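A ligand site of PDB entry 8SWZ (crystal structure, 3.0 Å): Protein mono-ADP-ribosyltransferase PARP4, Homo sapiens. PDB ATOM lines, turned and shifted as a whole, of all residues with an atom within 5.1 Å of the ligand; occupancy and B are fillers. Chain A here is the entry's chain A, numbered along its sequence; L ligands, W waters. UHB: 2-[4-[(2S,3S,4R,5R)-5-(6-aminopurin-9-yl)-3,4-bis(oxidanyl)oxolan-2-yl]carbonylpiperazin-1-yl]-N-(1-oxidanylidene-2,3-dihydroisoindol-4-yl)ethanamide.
An oxygen (O10) of the ligand sits close to the backbone carbonyl oxygen (O) of Leu 123, 3.3 Å away. Asn 130 touches the ligand. Arg 137 touches the ligand. CA of Leu 139 touches N34 of the ligand, 3.6 Å away. CB of Pro 142 touches C19 of the ligand, 3.8 Å away. Gly 161 touches the ligand. Tyr 163 touches the ligand (CB to C04, 3.2 Å). Glu 233 touches the ligand (CG to C02, 3.9 Å). Hydrophobic or aromatic side chains within 4 Å of the ligand: His 124, Ile 134, Leu 139, Leu 140, Pro 142, Tyr 163 and Tyr 174. Of the 23 residues printed, 17 come within 4 Å of the ligand. The nearest printed residue that does not touch the ligand is Gly 156 (4.2 Å).
Water W1 bridges an oxygen (O13) of the ligand (2.7 Å) and the side-chain hydroxyl (OH) of Tyr 174 (3.4 Å).
A ring nitrogen (ND1) of His 124 is in hydrogen-bond range of the backbone carbonyl oxygen (O) of Tyr 163 (2.7 Å). The backbone carbonyl oxygen of Ser 165 sits at hydrogen-bond distance from the backbone NH of Leu 123 (2.7 Å). The side-chain hydroxyl (OG) of Ser 126 is in hydrogen-bond range of the side-chain amide nitrogen (ND2) of Asn 130, 3.2 Å away. OG of Ser 171 sits close to O of Leu 123.
A ring nitrogen (NE2) of His 124 is in hydrogen-bond range of an oxygen (O29) of the ligand (3.1 Å). The side-chain hydroxyl of Ser 171 is in hydrogen-bond range of an oxygen (O10) of the ligand (2.9 Å). A nitrogen (N39) of the ligand is in hydrogen-bond range of the backbone carbonyl oxygen (O) of Gly 138. OH of Tyr 174 lies close to O13 of the ligand (3.3 Å). The backbone NH (N) of Ile 134 sits at hydrogen-bond distance from a nitrogen (N35) of the ligand, at 3.1 Å. The backbone carbonyl oxygen of Gly 133 is in hydrogen-bond range of a nitrogen (N39) of the ligand. The backbone NH (N) of Leu 140 is in hydrogen-bond range of a nitrogen (N34) of the ligand (2.7 Å). A nitrogen (N09) of the ligand is in hydrogen-bond range of the backbone carbonyl oxygen (O) of Gly 125. OG of Ser 126 lies within hydrogen-bond range of O29 of the ligand, 2.6 Å away. N of Gly 125 is in hydrogen-bond range of O10 of the ligand, 2.9 Å away.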
ATOM      1  N   LEU A 123      -1.303  -9.235  -1.410  1.00  0.00           N
ATOM      2  CA  LEU A 123      -2.607  -9.890  -1.276  1.00  0.00           C
ATOM      3  C   LEU A 123      -2.616 -10.981  -0.231  1.00  0.00           C
ATOM      4  O   LEU A 123      -1.810 -11.919  -0.280  1.00  0.00           O
ATOM      5  CB  LEU A 123      -3.021 -10.512  -2.606  1.00  0.00           C
ATOM      6  CG  LEU A 123      -2.932  -9.641  -3.839  1.00  0.00           C
ATOM      7  CD1 LEU A 123      -3.197 -10.531  -5.010  1.00  0.00           C
ATOM      8  CD2 LEU A 123      -3.978  -8.572  -3.747  1.00  0.00           C
ATOM      9  N   HIS A 124      -3.616 -10.965   0.631  1.00  0.00           N
ATOM     10  CA  HIS A 124      -3.840 -12.045   1.590  1.00  0.00           C
ATOM     11  C   HIS A 124      -5.245 -12.572   1.395  1.00  0.00           C
ATOM     12  O   HIS A 124      -6.223 -11.823   1.546  1.00  0.00           O
ATOM     13  CB  HIS A 124      -3.654 -11.547   3.017  1.00  0.00           C
ATOM     14  CG  HIS A 124      -3.905 -12.595   4.045  1.00  0.00           C
ATOM     15  ND1 HIS A 124      -2.910 -13.416   4.513  1.00  0.00           N
ATOM     16  CD2 HIS A 124      -5.038 -12.968   4.682  1.00  0.00           C
ATOM     17  CE1 HIS A 124      -3.406 -14.234   5.418  1.00  0.00           C
ATOM     18  NE2 HIS A 124      -4.697 -13.983   5.539  1.00  0.00           N
ATOM     19  N   GLY A 125      -5.351 -13.822   1.008  1.00  0.00           N
ATOM     20  CA  GLY A 125      -6.636 -14.462   0.879  1.00  0.00           C
ATOM     21  C   GLY A 125      -6.978 -15.176   2.159  1.00  0.00           C
ATOM     22  O   GLY A 125      -6.094 -15.581   2.904  1.00  0.00           O
ATOM     23  N   SER A 126      -8.281 -15.315   2.412  1.00  0.00           N
ATOM     24  CA  SER A 126      -8.763 -16.017   3.587  1.00  0.00           C
ATOM     25  C   SER A 126     -10.193 -16.437   3.350  1.00  0.00           C
ATOM     26  O   SER A 126     -10.949 -15.710   2.694  1.00  0.00           O
ATOM     27  CB  SER A 126      -8.691 -15.135   4.845  1.00  0.00           C
ATOM     28  OG  SER A 126      -8.829 -15.929   5.998  1.00  0.00           O
ATOM     29  N   PRO A 127     -10.615 -17.579   3.898  1.00  0.00           N
ATOM     30  CA  PRO A 127     -12.018 -17.964   3.763  1.00  0.00           C
ATOM     31  C   PRO A 127     -12.906 -16.898   4.375  1.00  0.00           C
ATOM     32  O   PRO A 127     -12.519 -16.168   5.291  1.00  0.00           O
ATOM     33  CB  PRO A 127     -12.115 -19.266   4.539  1.00  0.00           C
ATOM     34  CG  PRO A 127     -10.869 -19.328   5.341  1.00  0.00           C
ATOM     35  CD  PRO A 127      -9.838 -18.598   4.582  1.00  0.00           C
ATOM     36  N   ASN A 130     -13.543 -16.082   8.103  1.00  0.00           N
ATOM     37  CA  ASN A 130     -12.505 -15.456   8.900  1.00  0.00           C
ATOM     38  C   ASN A 130     -12.538 -13.941   8.856  1.00  0.00           C
ATOM     39  O   ASN A 130     -11.812 -13.317   9.627  1.00  0.00           O
ATOM     40  CB  ASN A 130     -11.136 -15.901   8.437  1.00  0.00           C
ATOM     41  CG  ASN A 130     -10.831 -17.245   8.872  1.00  0.00           C
ATOM     42  OD1 ASN A 130     -11.283 -17.655   9.924  1.00  0.00           O
ATOM     43  ND2 ASN A 130     -10.050 -17.972   8.093  1.00  0.00           N
ATOM     44  N   GLY A 133     -13.304 -12.014  12.040  1.00  0.00           N
ATOM     45  CA  GLY A 133     -12.165 -12.105  12.931  1.00  0.00           C
ATOM     46  C   GLY A 133     -11.012 -11.214  12.512  1.00  0.00           C
ATOM     47  O   GLY A 133     -10.376 -10.566  13.355  1.00  0.00           O
ATOM     48  N   ILE A 134     -10.716 -11.170  11.211  1.00  0.00           N
ATOM     49  CA  ILE A 134      -9.573 -10.425  10.704  1.00  0.00           C
ATOM     50  C   ILE A 134      -9.806  -8.930  10.826  1.00  0.00           C
ATOM     51  O   ILE A 134      -8.892  -8.187  11.158  1.00  0.00           O
ATOM     52  CB  ILE A 134      -9.263 -10.842   9.253  1.00  0.00           C
ATOM     53  CG1 ILE A 134      -8.823 -12.312   9.209  1.00  0.00           C
ATOM     54  CG2 ILE A 134      -8.218  -9.935   8.671  1.00  0.00           C
ATOM     55  CD1 ILE A 134      -8.661 -12.953   7.839  1.00  0.00           C
ATOM     56  N   ARG A 137      -9.516  -7.912  14.763  1.00  0.00           N
ATOM     57  CA  ARG A 137      -8.240  -8.113  15.447  1.00  0.00           C
ATOM     58  C   ARG A 137      -7.019  -7.949  14.560  1.00  0.00           C
ATOM     59  O   ARG A 137      -5.896  -8.014  15.083  1.00  0.00           O
ATOM     60  CB  ARG A 137      -8.189  -9.511  16.082  1.00  0.00           C
ATOM     61  CG  ARG A 137      -9.155  -9.776  17.229  1.00  0.00           C
ATOM     62  CD  ARG A 137      -8.570  -9.308  18.573  1.00  0.00           C
ATOM     63  NE  ARG A 137      -7.465 -10.158  18.996  1.00  0.00           N
ATOM     64  CZ  ARG A 137      -7.584 -11.201  19.811  1.00  0.00           C
ATOM     65  NH1 ARG A 137      -8.742 -11.532  20.361  1.00  0.00           N
ATOM     66  NH2 ARG A 137      -6.508 -11.946  20.077  1.00  0.00           N
ATOM     67  N   GLY A 138      -7.186  -7.639  13.286  1.00  0.00           N
ATOM     68  CA  GLY A 138      -6.069  -7.569  12.379  1.00  0.00           C
ATOM     69  C   GLY A 138      -5.633  -8.958  11.988  1.00  0.00           C
ATOM     70  O   GLY A 138      -6.279  -9.935  12.304  1.00  0.00           O
ATOM     71  N   LEU A 139      -4.552  -9.041  11.235  1.00  0.00           N
ATOM     72  CA  LEU A 139      -4.005 -10.326  10.836  1.00  0.00           C
ATOM     73  C   LEU A 139      -3.065 -10.861  11.933  1.00  0.00           C
ATOM     74  O   LEU A 139      -2.053 -10.217  12.235  1.00  0.00           O
ATOM     75  CB  LEU A 139      -3.277 -10.199   9.507  1.00  0.00           C
ATOM     76  CG  LEU A 139      -4.228 -10.296   8.341  1.00  0.00           C
ATOM     77  CD1 LEU A 139      -3.497  -9.857   7.142  1.00  0.00           C
ATOM     78  CD2 LEU A 139      -4.686 -11.720   8.201  1.00  0.00           C
ATOM     79  N   LEU A 140      -3.423 -11.997  12.543  1.00  0.00           N
ATOM     80  CA  LEU A 140      -2.721 -12.564  13.699  1.00  0.00           C
ATOM     81  C   LEU A 140      -1.695 -13.620  13.295  1.00  0.00           C
ATOM     82  O   LEU A 140      -1.840 -14.306  12.279  1.00  0.00           O
ATOM     83  CB  LEU A 140      -3.716 -13.169  14.700  1.00  0.00           C
ATOM     84  CG  LEU A 140      -4.670 -12.111  15.300  1.00  0.00           C
ATOM     85  CD1 LEU A 140      -5.656 -12.707  16.251  1.00  0.00           C
ATOM     86  CD2 LEU A 140      -3.982 -10.918  15.949  1.00  0.00           C
ATOM     87  N   LEU A 141      -0.634 -13.717  14.089  1.00  0.00           N
ATOM     88  CA  LEU A 141       0.332 -14.792  13.950  1.00  0.00           C
ATOM     89  C   LEU A 141      -0.313 -16.125  14.338  1.00  0.00           C
ATOM     90  O   LEU A 141      -1.149 -16.180  15.247  1.00  0.00           O
ATOM     91  CB  LEU A 141       1.543 -14.559  14.855  1.00  0.00           C
ATOM     92  CG  LEU A 141       2.450 -13.331  14.718  1.00  0.00           C
ATOM     93  CD1 LEU A 141       3.671 -13.480  15.548  1.00  0.00           C
ATOM     94  CD2 LEU A 141       2.875 -13.168  13.324  1.00  0.00           C
ATOM     95  N   PRO A 142       0.014 -17.220  13.660  1.00  0.00           N
ATOM     96  CA  PRO A 142      -0.483 -18.516  14.108  1.00  0.00           C
ATOM     97  C   PRO A 142       0.203 -18.890  15.403  1.00  0.00           C
ATOM     98  O   PRO A 142       1.258 -18.340  15.726  1.00  0.00           O
ATOM     99  CB  PRO A 142      -0.082 -19.455  12.968  1.00  0.00           C
ATOM    100  CG  PRO A 142       1.173 -18.849  12.445  1.00  0.00           C
ATOM    101  CD  PRO A 142       0.980 -17.350  12.565  1.00  0.00           C
ATOM    102  N   GLY A 156       2.845 -23.230   7.846  1.00  0.00           N
ATOM    103  CA  GLY A 156       2.978 -23.112   6.420  1.00  0.00           C
ATOM    104  C   GLY A 156       4.383 -23.510   5.982  1.00  0.00           C
ATOM    105  O   GLY A 156       5.218 -23.929   6.792  1.00  0.00           O
ATOM    106  N   GLY A 161       4.269 -17.450  10.642  1.00  0.00           N
ATOM    107  CA  GLY A 161       4.198 -16.041  10.296  1.00  0.00           C
ATOM    108  C   GLY A 161       2.948 -15.656   9.525  1.00  0.00           C
ATOM    109  O   GLY A 161       2.058 -16.485   9.338  1.00  0.00           O
ATOM    110  N   TYR A 163       1.293 -14.586   6.006  1.00  0.00           N
ATOM    111  CA  TYR A 163       1.636 -14.917   4.635  1.00  0.00           C
ATOM    112  C   TYR A 163       0.893 -14.028   3.641  1.00  0.00           C
ATOM    113  O   TYR A 163      -0.335 -13.911   3.715  1.00  0.00           O
ATOM    114  CB  TYR A 163       1.286 -16.373   4.350  1.00  0.00           C
ATOM    115  CG  TYR A 163       2.202 -17.402   4.947  1.00  0.00           C
ATOM    116  CD1 TYR A 163       2.305 -17.567   6.312  1.00  0.00           C
ATOM    117  CD2 TYR A 163       2.965 -18.220   4.136  1.00  0.00           C
ATOM    118  CE1 TYR A 163       3.168 -18.518   6.864  1.00  0.00           C
ATOM    119  CE2 TYR A 163       3.820 -19.175   4.660  1.00  0.00           C
ATOM    120  CZ  TYR A 163       3.918 -19.321   6.013  1.00  0.00           C
ATOM    121  OH  TYR A 163       4.773 -20.262   6.517  1.00  0.00           O
ATOM    122  N   PHE A 164       1.619 -13.506   2.667  1.00  0.00           N
ATOM    123  CA  PHE A 164       1.056 -12.719   1.579  1.00  0.00           C
ATOM    124  C   PHE A 164       1.573 -13.238   0.255  1.00  0.00           C
ATOM    125  O   PHE A 164       2.573 -13.944   0.187  1.00  0.00           O
ATOM    126  CB  PHE A 164       1.438 -11.239   1.695  1.00  0.00           C
ATOM    127  CG  PHE A 164       1.002 -10.588   2.967  1.00  0.00           C
ATOM    128  CD1 PHE A 164       1.786 -10.647   4.080  1.00  0.00           C
ATOM    129  CD2 PHE A 164      -0.174  -9.883   3.015  1.00  0.00           C
ATOM    130  CE1 PHE A 164       1.379 -10.040   5.238  1.00  0.00           C
ATOM    131  CE2 PHE A 164      -0.583  -9.274   4.159  1.00  0.00           C
ATOM    132  CZ  PHE A 164       0.194  -9.353   5.278  1.00  0.00           C
ATOM    133  N   SER A 165       0.884 -12.863  -0.825  1.00  0.00           N
ATOM    134  CA  SER A 165       1.435 -13.019  -2.165  1.00  0.00           C
ATOM    135  C   SER A 165       1.248 -11.741  -2.978  1.00  0.00           C
ATOM    136  O   SER A 165       0.430 -10.867  -2.649  1.00  0.00           O
ATOM    137  CB  SER A 165       0.790 -14.162  -2.938  1.00  0.00           C
ATOM    138  OG  SER A 165       1.414 -14.267  -4.219  1.00  0.00           O
ATOM    139  N   THR A 170      -2.315 -16.922  -6.806  1.00  0.00           N
ATOM    140  CA  THR A 170      -2.109 -17.733  -5.609  1.00  0.00           C
ATOM    141  C   THR A 170      -3.102 -17.391  -4.494  1.00  0.00           C
ATOM    142  O   THR A 170      -3.478 -18.268  -3.703  1.00  0.00           O
ATOM    143  CB  THR A 170      -0.624 -17.671  -5.190  1.00  0.00           C
ATOM    144  OG1 THR A 170      -0.195 -16.326  -4.915  1.00  0.00           O
ATOM    145  CG2 THR A 170       0.292 -18.326  -6.238  1.00  0.00           C
ATOM    146  N   SER A 171      -3.576 -16.148  -4.412  1.00  0.00           N
ATOM    147  CA  SER A 171      -4.533 -15.807  -3.363  1.00  0.00           C
ATOM    148  C   SER A 171      -5.879 -16.465  -3.598  1.00  0.00           C
ATOM    149  O   SER A 171      -6.602 -16.745  -2.637  1.00  0.00           O
ATOM    150  CB  SER A 171      -4.660 -14.299  -3.246  1.00  0.00           C
ATOM    151  OG  SER A 171      -3.481 -13.802  -2.629  1.00  0.00           O
ATOM    152  N   TYR A 174      -6.447 -19.555  -1.494  1.00  0.00           N
ATOM    153  CA  TYR A 174      -6.804 -19.389  -0.078  1.00  0.00           C
ATOM    154  C   TYR A 174      -8.108 -18.620   0.128  1.00  0.00           C
ATOM    155  O   TYR A 174      -8.680 -18.671   1.237  1.00  0.00           O
ATOM    156  CB  TYR A 174      -5.672 -18.672   0.696  1.00  0.00           C
ATOM    157  CG  TYR A 174      -4.334 -19.372   0.618  1.00  0.00           C
ATOM    158  CD1 TYR A 174      -3.428 -19.091  -0.395  1.00  0.00           C
ATOM    159  CD2 TYR A 174      -3.963 -20.326   1.553  1.00  0.00           C
ATOM    160  CE1 TYR A 174      -2.202 -19.744  -0.476  1.00  0.00           C
ATOM    161  CE2 TYR A 174      -2.731 -20.986   1.492  1.00  0.00           C
ATOM    162  CZ  TYR A 174      -1.860 -20.699   0.467  1.00  0.00           C
ATOM    163  OH  TYR A 174      -0.637 -21.336   0.388  1.00  0.00           O
ATOM    164  N   GLU A 233       5.743 -16.463  -2.021  1.00  0.00           N
ATOM    165  CA  GLU A 233       5.192 -16.305  -0.696  1.00  0.00           C
ATOM    166  C   GLU A 233       6.027 -15.264   0.041  1.00  0.00           C
ATOM    167  O   GLU A 233       7.259 -15.306  -0.002  1.00  0.00           O
ATOM    168  CB  GLU A 233       5.184 -17.633   0.072  1.00  0.00           C
ATOM    169  CG  GLU A 233       4.072 -18.583  -0.347  1.00  0.00           C
ATOM    170  CD  GLU A 233       4.219 -20.009   0.208  1.00  0.00           C
ATOM    171  OE1 GLU A 233       5.042 -20.235   1.121  1.00  0.00           O
ATOM    172  OE2 GLU A 233       3.408 -20.879  -0.203  1.00  0.00           O
HETATM  173  C01 UHB L   1      -0.440 -16.902   0.342  1.00  0.00           C
HETATM  174  C02 UHB L   1       0.456 -17.862   0.791  1.00  0.00           C
HETATM  175  C03 UHB L   1       0.260 -18.527   1.999  1.00  0.00           C
HETATM  176  C04 UHB L   1      -0.837 -18.245   2.798  1.00  0.00           C
HETATM  177  C05 UHB L   1      -1.738 -17.281   2.357  1.00  0.00           C
HETATM  178  C06 UHB L   1      -1.530 -16.627   1.162  1.00  0.00           C
HETATM  179  C07 UHB L   1      -2.632 -15.674   0.958  1.00  0.00           C
HETATM  180  C08 UHB L   1      -2.995 -16.775   2.999  1.00  0.00           C
HETATM  181  N09 UHB L   1      -3.327 -15.672   2.130  1.00  0.00           N
HETATM  182  O10 UHB L   1      -2.905 -15.006  -0.045  1.00  0.00           O
HETATM  183  N11 UHB L   1      -1.026 -18.917   4.025  1.00  0.00           N
HETATM  184  C12 UHB L   1      -0.487 -20.102   4.388  1.00  0.00           C
HETATM  185  O13 UHB L   1      -0.470 -21.089   3.669  1.00  0.00           O
HETATM  186  C14 UHB L   1       0.121 -20.130   5.771  1.00  0.00           C
HETATM  187  N15 UHB L   1      -0.805 -19.722   6.819  1.00  0.00           N
HETATM  188  C16 UHB L   1      -1.854 -20.731   7.004  1.00  0.00           C
HETATM  189  C17 UHB L   1      -2.975 -20.175   7.859  1.00  0.00           C
HETATM  190  N18 UHB L   1      -2.412 -19.300   8.890  1.00  0.00           N
HETATM  191  C19 UHB L   1      -1.054 -19.674   9.263  1.00  0.00           C
HETATM  192  C20 UHB L   1      -0.114 -19.506   8.085  1.00  0.00           C
HETATM  193  C21 UHB L   1      -3.053 -18.278   9.447  1.00  0.00           C
HETATM  194  C22 UHB L   1      -4.495 -18.046   9.089  1.00  0.00           C
HETATM  195  C23 UHB L   1      -4.667 -17.232   7.799  1.00  0.00           C
HETATM  196  C24 UHB L   1      -5.493 -15.990   8.172  1.00  0.00           C
HETATM  197  C25 UHB L   1      -6.049 -16.370   9.540  1.00  0.00           C
HETATM  198  O26 UHB L   1      -5.127 -17.282  10.121  1.00  0.00           O
HETATM  199  O27 UHB L   1      -2.509 -17.533  10.249  1.00  0.00           O
HETATM  200  O28 UHB L   1      -5.337 -18.015   6.835  1.00  0.00           O
HETATM  201  O29 UHB L   1      -6.528 -15.733   7.253  1.00  0.00           O
HETATM  202  N30 UHB L   1      -6.176 -15.230  10.447  1.00  0.00           N
HETATM  203  C31 UHB L   1      -6.944 -13.693  11.808  1.00  0.00           C
HETATM  204  C32 UHB L   1      -7.325 -14.778  11.056  1.00  0.00           C
HETATM  205  C33 UHB L   1      -5.177 -14.393  10.851  1.00  0.00           C
HETATM  206  N34 UHB L   1      -5.582 -13.454  11.671  1.00  0.00           N
HETATM  207  N35 UHB L   1      -9.199 -13.528  12.456  1.00  0.00           N
HETATM  208  C36 UHB L   1      -9.417 -14.597  11.683  1.00  0.00           C
HETATM  209  N37 UHB L   1      -8.559 -15.289  10.947  1.00  0.00           N
HETATM  210  C38 UHB L   1      -7.945 -13.034  12.548  1.00  0.00           C
HETATM  211  N39 UHB L   1      -7.729 -11.976  13.313  1.00  0.00           N
HETATM  212  O   HOH W   1       1.285 -22.859   2.740  1.00  0.00           O
